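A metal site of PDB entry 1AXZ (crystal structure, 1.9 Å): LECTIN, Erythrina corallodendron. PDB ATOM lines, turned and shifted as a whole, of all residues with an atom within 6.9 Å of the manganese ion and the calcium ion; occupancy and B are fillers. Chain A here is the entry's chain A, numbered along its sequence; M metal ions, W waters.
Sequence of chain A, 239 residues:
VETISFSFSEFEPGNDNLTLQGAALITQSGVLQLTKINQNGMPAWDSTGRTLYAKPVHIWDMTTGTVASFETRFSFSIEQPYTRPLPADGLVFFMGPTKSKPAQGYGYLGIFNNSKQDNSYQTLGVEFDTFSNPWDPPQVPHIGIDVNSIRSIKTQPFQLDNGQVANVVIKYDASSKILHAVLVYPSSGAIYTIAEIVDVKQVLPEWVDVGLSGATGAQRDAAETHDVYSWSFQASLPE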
ATOM      1  N   ASP A  89      34.600  -8.847   0.166  1.00  0.00           N
ATOM      2  CA  ASP A  89      33.492  -8.768   1.111  1.00  0.00           C
ATOM      3  C   ASP A  89      33.768  -9.540   2.411  1.00  0.00           C
ATOM      4  O   ASP A  89      33.166  -9.240   3.443  1.00  0.00           O
ATOM      5  CB  ASP A  89      32.210  -9.321   0.477  1.00  0.00           C
ATOM      6  CG  ASP A  89      31.387  -8.248  -0.195  1.00  0.00           C
ATOM      7  OD1 ASP A  89      30.734  -7.459   0.515  1.00  0.00           O
ATOM      8  OD2 ASP A  89      31.393  -8.200  -1.437  1.00  0.00           O
ATOM      9  N   GLY A  90      34.619 -10.549   2.325  1.00  0.00           N
ATOM     10  CA  GLY A  90      34.965 -11.321   3.507  1.00  0.00           C
ATOM     11  C   GLY A  90      34.992 -12.823   3.302  1.00  0.00           C
ATOM     12  O   GLY A  90      34.876 -13.304   2.175  1.00  0.00           O
ATOM     13  N   TYR A 106      29.173 -11.623  -3.044  1.00  0.00           N
ATOM     14  CA  TYR A 106      29.213 -10.299  -2.431  1.00  0.00           C
ATOM     15  C   TYR A 106      28.990 -10.386  -0.916  1.00  0.00           C
ATOM     16  O   TYR A 106      29.566 -11.249  -0.252  1.00  0.00           O
ATOM     17  CB  TYR A 106      28.169  -9.370  -3.082  1.00  0.00           C
ATOM     18  CG  TYR A 106      28.192  -9.406  -4.599  1.00  0.00           C
ATOM     19  CD1 TYR A 106      29.397  -9.432  -5.301  1.00  0.00           C
ATOM     20  CD2 TYR A 106      27.009  -9.438  -5.330  1.00  0.00           C
ATOM     21  CE1 TYR A 106      29.425  -9.499  -6.684  1.00  0.00           C
ATOM     22  CE2 TYR A 106      27.015  -9.506  -6.716  1.00  0.00           C
ATOM     23  CZ  TYR A 106      28.229  -9.532  -7.388  1.00  0.00           C
ATOM     24  OH  TYR A 106      28.243  -9.615  -8.760  1.00  0.00           O
ATOM     25  N   GLY A 107      28.164  -9.488  -0.382  1.00  0.00           N
ATOM     26  CA  GLY A 107      27.879  -9.467   1.038  1.00  0.00           C
ATOM     27  C   GLY A 107      27.222 -10.714   1.609  1.00  0.00           C
ATOM     28  O   GLY A 107      27.158 -10.869   2.834  1.00  0.00           O
ATOM     29  N   TYR A 108      26.711 -11.579   0.745  1.00  0.00           N
ATOM     30  CA  TYR A 108      26.067 -12.818   1.189  1.00  0.00           C
ATOM     31  C   TYR A 108      27.099 -13.916   1.420  1.00  0.00           C
ATOM     32  O   TYR A 108      26.782 -15.008   1.882  1.00  0.00           O
ATOM     33  CB  TYR A 108      24.992 -13.258   0.200  1.00  0.00           C
ATOM     34  CG  TYR A 108      23.919 -12.205   0.047  1.00  0.00           C
ATOM     35  CD1 TYR A 108      23.142 -11.818   1.123  1.00  0.00           C
ATOM     36  CD2 TYR A 108      23.723 -11.562  -1.183  1.00  0.00           C
ATOM     37  CE1 TYR A 108      22.192 -10.800   1.001  1.00  0.00           C
ATOM     38  CE2 TYR A 108      22.774 -10.553  -1.309  1.00  0.00           C
ATOM     39  CZ  TYR A 108      22.013 -10.171  -0.219  1.00  0.00           C
ATOM     40  OH  TYR A 108      21.081  -9.176  -0.334  1.00  0.00           O
ATOM     41  N   LEU A 109      28.338 -13.613   1.039  1.00  0.00           N
ATOM     42  CA  LEU A 109      29.486 -14.494   1.237  1.00  0.00           C
ATOM     43  C   LEU A 109      29.442 -15.897   0.630  1.00  0.00           C
ATOM     44  O   LEU A 109      30.216 -16.770   1.032  1.00  0.00           O
ATOM     45  CB  LEU A 109      29.794 -14.588   2.737  1.00  0.00           C
ATOM     46  CG  LEU A 109      29.933 -13.230   3.449  1.00  0.00           C
ATOM     47  CD1 LEU A 109      30.085 -13.435   4.957  1.00  0.00           C
ATOM     48  CD2 LEU A 109      31.125 -12.458   2.882  1.00  0.00           C
ATOM     49  N   GLU A 127      31.520 -15.586  10.424  1.00  0.00           N
ATOM     50  CA  GLU A 127      32.078 -14.733   9.386  1.00  0.00           C
ATOM     51  C   GLU A 127      33.139 -13.758   9.862  1.00  0.00           C
ATOM     52  O   GLU A 127      33.199 -13.397  11.035  1.00  0.00           O
ATOM     53  CB  GLU A 127      30.964 -13.921   8.743  1.00  0.00           C
ATOM     54  CG  GLU A 127      30.222 -13.093   9.773  1.00  0.00           C
ATOM     55  CD  GLU A 127      29.318 -12.052   9.165  1.00  0.00           C
ATOM     56  OE1 GLU A 127      28.452 -12.405   8.354  1.00  0.00           O
ATOM     57  OE2 GLU A 127      29.501 -10.884   9.519  1.00  0.00           O
ATOM     58  N   PHE A 128      33.957 -13.343   8.892  1.00  0.00           N
ATOM     59  CA  PHE A 128      35.031 -12.368   9.069  1.00  0.00           C
ATOM     60  C   PHE A 128      34.724 -11.438   7.907  1.00  0.00           C
ATOM     61  O   PHE A 128      35.142 -11.625   6.771  1.00  0.00           O
ATOM     62  CB  PHE A 128      36.388 -13.076   8.953  1.00  0.00           C
ATOM     63  CG  PHE A 128      36.581 -14.117  10.018  1.00  0.00           C
ATOM     64  CD1 PHE A 128      37.081 -13.752  11.270  1.00  0.00           C
ATOM     65  CD2 PHE A 128      36.165 -15.428   9.815  1.00  0.00           C
ATOM     66  CE1 PHE A 128      37.171 -14.694  12.308  1.00  0.00           C
ATOM     67  CE2 PHE A 128      36.242 -16.369  10.847  1.00  0.00           C
ATOM     68  CZ  PHE A 128      36.748 -15.999  12.088  1.00  0.00           C
ATOM     69  N   ASP A 129      33.834 -10.504   8.229  1.00  0.00           N
ATOM     70  CA  ASP A 129      33.275  -9.531   7.316  1.00  0.00           C
ATOM     71  C   ASP A 129      34.061  -8.232   7.189  1.00  0.00           C
ATOM     72  O   ASP A 129      34.221  -7.508   8.172  1.00  0.00           O
ATOM     73  CB  ASP A 129      31.875  -9.233   7.808  1.00  0.00           C
ATOM     74  CG  ASP A 129      31.012  -8.589   6.768  1.00  0.00           C
ATOM     75  OD1 ASP A 129      31.521  -8.042   5.785  1.00  0.00           O
ATOM     76  OD2 ASP A 129      29.800  -8.666   6.938  1.00  0.00           O
ATOM     77  N   THR A 130      34.392  -7.880   5.954  1.00  0.00           N
ATOM     78  CA  THR A 130      35.186  -6.687   5.685  1.00  0.00           C
ATOM     79  C   THR A 130      34.462  -5.481   5.078  1.00  0.00           C
ATOM     80  O   THR A 130      35.060  -4.411   4.919  1.00  0.00           O
ATOM     81  CB  THR A 130      36.366  -7.037   4.761  1.00  0.00           C
ATOM     82  OG1 THR A 130      35.865  -7.628   3.562  1.00  0.00           O
ATOM     83  CG2 THR A 130      37.298  -8.033   5.453  1.00  0.00           C
ATOM     84  N   PHE A 131      33.189  -5.655   4.716  1.00  0.00           N
ATOM     85  CA  PHE A 131      32.426  -4.554   4.121  1.00  0.00           C
ATOM     86  C   PHE A 131      31.097  -4.362   4.841  1.00  0.00           C
ATOM     87  O   PHE A 131      30.351  -5.320   5.042  1.00  0.00           O
ATOM     88  CB  PHE A 131      32.176  -4.828   2.634  1.00  0.00           C
ATOM     89  CG  PHE A 131      31.432  -3.717   1.934  1.00  0.00           C
ATOM     90  CD1 PHE A 131      30.039  -3.714   1.920  1.00  0.00           C
ATOM     91  CD2 PHE A 131      32.117  -2.677   1.322  1.00  0.00           C
ATOM     92  CE1 PHE A 131      29.335  -2.675   1.302  1.00  0.00           C
ATOM     93  CE2 PHE A 131      31.423  -1.636   0.702  1.00  0.00           C
ATOM     94  CZ  PHE A 131      30.034  -1.636   0.696  1.00  0.00           C
ATOM     95  N   SER A 132      30.777  -3.127   5.199  1.00  0.00           N
ATOM     96  CA  SER A 132      29.524  -2.859   5.907  1.00  0.00           C
ATOM     97  C   SER A 132      28.310  -2.704   4.995  1.00  0.00           C
ATOM     98  O   SER A 132      28.149  -1.670   4.335  1.00  0.00           O
ATOM     99  CB  SER A 132      29.669  -1.616   6.801  1.00  0.00           C
ATOM    100  OG  SER A 132      28.530  -1.461   7.627  1.00  0.00           O
ATOM    101  N   ASN A 133      27.486  -3.745   4.925  1.00  0.00           N
ATOM    102  CA  ASN A 133      26.264  -3.734   4.133  1.00  0.00           C
ATOM    103  C   ASN A 133      25.162  -3.092   4.986  1.00  0.00           C
ATOM    104  O   ASN A 133      25.381  -2.818   6.168  1.00  0.00           O
ATOM    105  CB  ASN A 133      25.867  -5.165   3.744  1.00  0.00           C
ATOM    106  CG  ASN A 133      26.866  -5.831   2.821  1.00  0.00           C
ATOM    107  OD1 ASN A 133      27.756  -6.538   3.261  1.00  0.00           O
ATOM    108  ND2 ASN A 133      26.722  -5.600   1.522  1.00  0.00           N
ATOM    109  N   TRP A 135      22.676  -4.308   6.447  1.00  0.00           N
ATOM    110  CA  TRP A 135      22.295  -5.161   7.575  1.00  0.00           C
ATOM    111  C   TRP A 135      23.433  -5.317   8.584  1.00  0.00           C
ATOM    112  O   TRP A 135      23.290  -6.005   9.589  1.00  0.00           O
ATOM    113  CB  TRP A 135      21.885  -6.547   7.071  1.00  0.00           C
ATOM    114  CG  TRP A 135      22.939  -7.226   6.246  1.00  0.00           C
ATOM    115  CD1 TRP A 135      24.056  -7.876   6.698  1.00  0.00           C
ATOM    116  CD2 TRP A 135      22.988  -7.305   4.817  1.00  0.00           C
ATOM    117  NE1 TRP A 135      24.784  -8.360   5.640  1.00  0.00           N
ATOM    118  CE2 TRP A 135      24.146  -8.033   4.466  1.00  0.00           C
ATOM    119  CE3 TRP A 135      22.146  -6.849   3.792  1.00  0.00           C
ATOM    120  CZ2 TRP A 135      24.502  -8.303   3.143  1.00  0.00           C
ATOM    121  CZ3 TRP A 135      22.502  -7.118   2.469  1.00  0.00           C
ATOM    122  CH2 TRP A 135      23.673  -7.841   2.160  1.00  0.00           C
ATOM    123  N   ASP A 136      24.566  -4.688   8.283  1.00  0.00           N
ATOM    124  CA  ASP A 136      25.761  -4.751   9.122  1.00  0.00           C
ATOM    125  C   ASP A 136      25.948  -3.608  10.088  1.00  0.00           C
ATOM    126  O   ASP A 136      25.384  -2.526   9.908  1.00  0.00           O
ATOM    127  CB  ASP A 136      27.011  -4.756   8.240  1.00  0.00           C
ATOM    128  CG  ASP A 136      27.282  -6.088   7.627  1.00  0.00           C
ATOM    129  OD1 ASP A 136      26.974  -7.082   8.280  1.00  0.00           O
ATOM    130  OD2 ASP A 136      27.774  -6.153   6.496  1.00  0.00           O
ATOM    131  N   PRO A 137      26.727  -3.841  11.163  1.00  0.00           N
ATOM    132  CA  PRO A 137      26.991  -2.773  12.117  1.00  0.00           C
ATOM    133  C   PRO A 137      27.991  -1.903  11.343  1.00  0.00           C
ATOM    134  O   PRO A 137      28.640  -2.388  10.407  1.00  0.00           O
ATOM    135  CB  PRO A 137      27.664  -3.511  13.275  1.00  0.00           C
ATOM    136  CG  PRO A 137      28.322  -4.682  12.606  1.00  0.00           C
ATOM    137  CD  PRO A 137      27.258  -5.131  11.643  1.00  0.00           C
ATOM    138  N   VAL A 140      33.826  -2.263  10.618  1.00  0.00           N
ATOM    139  CA  VAL A 140      34.412  -3.335   9.819  1.00  0.00           C
ATOM    140  C   VAL A 140      35.929  -3.222   9.895  1.00  0.00           C
ATOM    141  O   VAL A 140      36.481  -2.135  10.009  1.00  0.00           O
ATOM    142  CB  VAL A 140      33.971  -3.308   8.324  1.00  0.00           C
ATOM    143  CG1 VAL A 140      32.534  -3.792   8.195  1.00  0.00           C
ATOM    144  CG2 VAL A 140      34.132  -1.902   7.742  1.00  0.00           C
ATOM    145  N   HIS A 142      34.637  -7.214  11.118  1.00  0.00           N
ATOM    146  CA  HIS A 142      34.061  -7.760  12.332  1.00  0.00           C
ATOM    147  C   HIS A 142      33.798  -9.249  12.198  1.00  0.00           C
ATOM    148  O   HIS A 142      33.645  -9.783  11.089  1.00  0.00           O
ATOM    149  CB  HIS A 142      32.766  -7.037  12.723  1.00  0.00           C
ATOM    150  CG  HIS A 142      31.703  -7.060  11.665  1.00  0.00           C
ATOM    151  ND1 HIS A 142      31.439  -6.006  10.826  1.00  0.00           N
ATOM    152  CD2 HIS A 142      30.833  -8.047  11.315  1.00  0.00           C
ATOM    153  CE1 HIS A 142      30.438  -6.380  10.013  1.00  0.00           C
ATOM    154  NE2 HIS A 142      30.047  -7.607  10.285  1.00  0.00           N
ATOM    155  N   ILE A 143      33.854  -9.920  13.337  1.00  0.00           N
ATOM    156  CA  ILE A 143      33.567 -11.339  13.407  1.00  0.00           C
ATOM    157  C   ILE A 143      32.077 -11.361  13.682  1.00  0.00           C
ATOM    158  O   ILE A 143      31.561 -10.500  14.399  1.00  0.00           O
ATOM    159  CB  ILE A 143      34.264 -12.018  14.612  1.00  0.00           C
ATOM    160  CG1 ILE A 143      35.766 -11.718  14.592  1.00  0.00           C
ATOM    161  CG2 ILE A 143      34.025 -13.531  14.573  1.00  0.00           C
ATOM    162  CD1 ILE A 143      36.498 -12.168  15.854  1.00  0.00           C
ATOM    163  N   GLY A 144      31.364 -12.320  13.100  1.00  0.00           N
ATOM    164  CA  GLY A 144      29.939 -12.399  13.340  1.00  0.00           C
ATOM    165  C   GLY A 144      29.466 -13.835  13.386  1.00  0.00           C
ATOM    166  O   GLY A 144      30.018 -14.700  12.710  1.00  0.00           O
ATOM    167  N   ASP A 146      26.488 -16.111  12.488  1.00  0.00           N
ATOM    168  CA  ASP A 146      25.313 -16.123  11.626  1.00  0.00           C
ATOM    169  C   ASP A 146      24.479 -17.378  11.798  1.00  0.00           C
ATOM    170  O   ASP A 146      24.951 -18.488  11.563  1.00  0.00           O
ATOM    171  CB  ASP A 146      25.749 -16.016  10.159  1.00  0.00           C
ATOM    172  CG  ASP A 146      26.594 -14.789   9.870  1.00  0.00           C
ATOM    173  OD1 ASP A 146      26.655 -13.881  10.721  1.00  0.00           O
ATOM    174  OD2 ASP A 146      27.212 -14.731   8.781  1.00  0.00           O
ATOM    175  N   ILE A 150      22.341 -13.695   7.194  1.00  0.00           N
ATOM    176  CA  ILE A 150      23.564 -12.911   7.039  1.00  0.00           C
ATOM    177  C   ILE A 150      23.553 -11.819   8.120  1.00  0.00           C
ATOM    178  O   ILE A 150      24.570 -11.172   8.381  1.00  0.00           O
ATOM    179  CB  ILE A 150      23.657 -12.319   5.611  1.00  0.00           C
ATOM    180  CG1 ILE A 150      25.068 -11.780   5.351  1.00  0.00           C
ATOM    181  CG2 ILE A 150      22.592 -11.241   5.396  1.00  0.00           C
ATOM    182  CD1 ILE A 150      26.147 -12.864   5.365  1.00  0.00           C
ATOM    183  N   ARG A 151      22.391 -11.615   8.735  1.00  0.00           N
ATOM    184  CA  ARG A 151      22.239 -10.637   9.806  1.00  0.00           C
ATOM    185  C   ARG A 151      22.648 -11.323  11.108  1.00  0.00           C
ATOM    186  O   ARG A 151      21.822 -11.945  11.780  1.00  0.00           O
ATOM    187  CB  ARG A 151      20.783 -10.154   9.900  1.00  0.00           C
ATOM    188  CG  ARG A 151      20.347  -9.286   8.732  1.00  0.00           C
ATOM    189  CD  ARG A 151      18.987  -8.655   8.990  1.00  0.00           C
ATOM    190  NE  ARG A 151      17.901  -9.444   8.421  1.00  0.00           N
ATOM    191  CZ  ARG A 151      16.853  -9.904   9.102  1.00  0.00           C
ATOM    192  NH1 ARG A 151      16.731  -9.662  10.403  1.00  0.00           N
ATOM    193  NH2 ARG A 151      15.921 -10.594   8.476  1.00  0.00           N
ATOM    194  N   SER A 152      23.915 -11.179  11.463  1.00  0.00           N
ATOM    195  CA  SER A 152      24.491 -11.817  12.649  1.00  0.00           C
ATOM    196  C   SER A 152      23.729 -11.581  13.948  1.00  0.00           C
ATOM    197  O   SER A 152      23.199 -10.499  14.184  1.00  0.00           O
ATOM    198  CB  SER A 152      25.932 -11.350  12.850  1.00  0.00           C
ATOM    199  OG  SER A 152      26.691 -11.501  11.663  1.00  0.00           O
ATOM    200  N   THR A 155      28.084  -9.717  16.959  1.00  0.00           N
ATOM    201  CA  THR A 155      29.225  -9.215  16.190  1.00  0.00           C
ATOM    202  C   THR A 155      30.337  -8.730  17.125  1.00  0.00           C
ATOM    203  O   THR A 155      30.075  -8.351  18.270  1.00  0.00           O
ATOM    204  CB  THR A 155      28.780  -8.043  15.260  1.00  0.00           C
ATOM    205  OG1 THR A 155      28.100  -8.579  14.105  1.00  0.00           O
ATOM    206  CG2 THR A 155      29.950  -7.224  14.787  1.00  0.00           C
HETATM  207 MN    MN M   1      28.464  -8.835   8.900  1.00  0.00          MN
HETATM  208 CA    CA M   2      29.174  -7.395   4.982  1.00  0.00          CA
HETATM  209  O   HOH W   1      26.939 -10.321   7.603  1.00  0.00           O
HETATM  210  O   HOH W   2      27.715  -9.363   4.978  1.00  0.00           O
HETATM  211  O   HOH W   3      27.013  -8.995  10.842  1.00  0.00           O
HETATM  212  O   HOH W   4      30.494  -8.184   3.096  1.00  0.00           O
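The backbone NH (N) of Glu 127 lies within hydrogen-bond range of the backbone carbonyl oxygen (O) of Gly 144, at 2.9 Å. The side-chain carboxylate (OE1) of Glu 127 lies close to the side-chain carboxylate (OD2) of Asp 146 (2.7 Å).
Four residues have an atom within 4 Å of the manganese ion: Glu 127, Asp 129, Asp 136 and His 142. Along chain A the residues within 4 Å of the manganese ion span positions 127 to 142.
Of the 25 residues printed, 4 come within 4 Å of the calcium ion. Along chain A the residues within 4 Å of the calcium ion span positions 129 to 136.
The manganese ion is bound by OE2 of Glu 127, OD2 of Asp 129, OD1 of Asp 136, water W3, NE2 of His 142 and water W1. The manganese ion has six donor atoms within binding distance.
The calcium ion is bound by the backbone carbonyl oxygen (O) of Phe 131 (2.4 Å), the side-chain amide oxygen (OD1) of Asn 133 (2.4 Å), the side-chain carboxylate (OD2) of Asp 136 (2.4 Å), the side-chain carboxylate (OD2) of Asp 129 (2.4 Å), water W4 (2.4 Å), water W2 (2.4 Å) and the side-chain carboxylate (OD1) of Asp 129 (2.6 Å). The calcium ion has seven donor atoms within binding distance.
Water W1 lies within hydrogen-bond range of O of Ile 150 (2.6 Å) and OE1 of Glu 127 (2.7 Å). Water W3 lies within hydrogen-bond range of the side-chain hydroxyl of Ser 152 and the side-chain hydroxyl of Thr 155. Water W2 lies within hydrogen-bond range of O of Gly 107 (2.7 Å) and NE1 of Trp 135 (3.2 Å).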
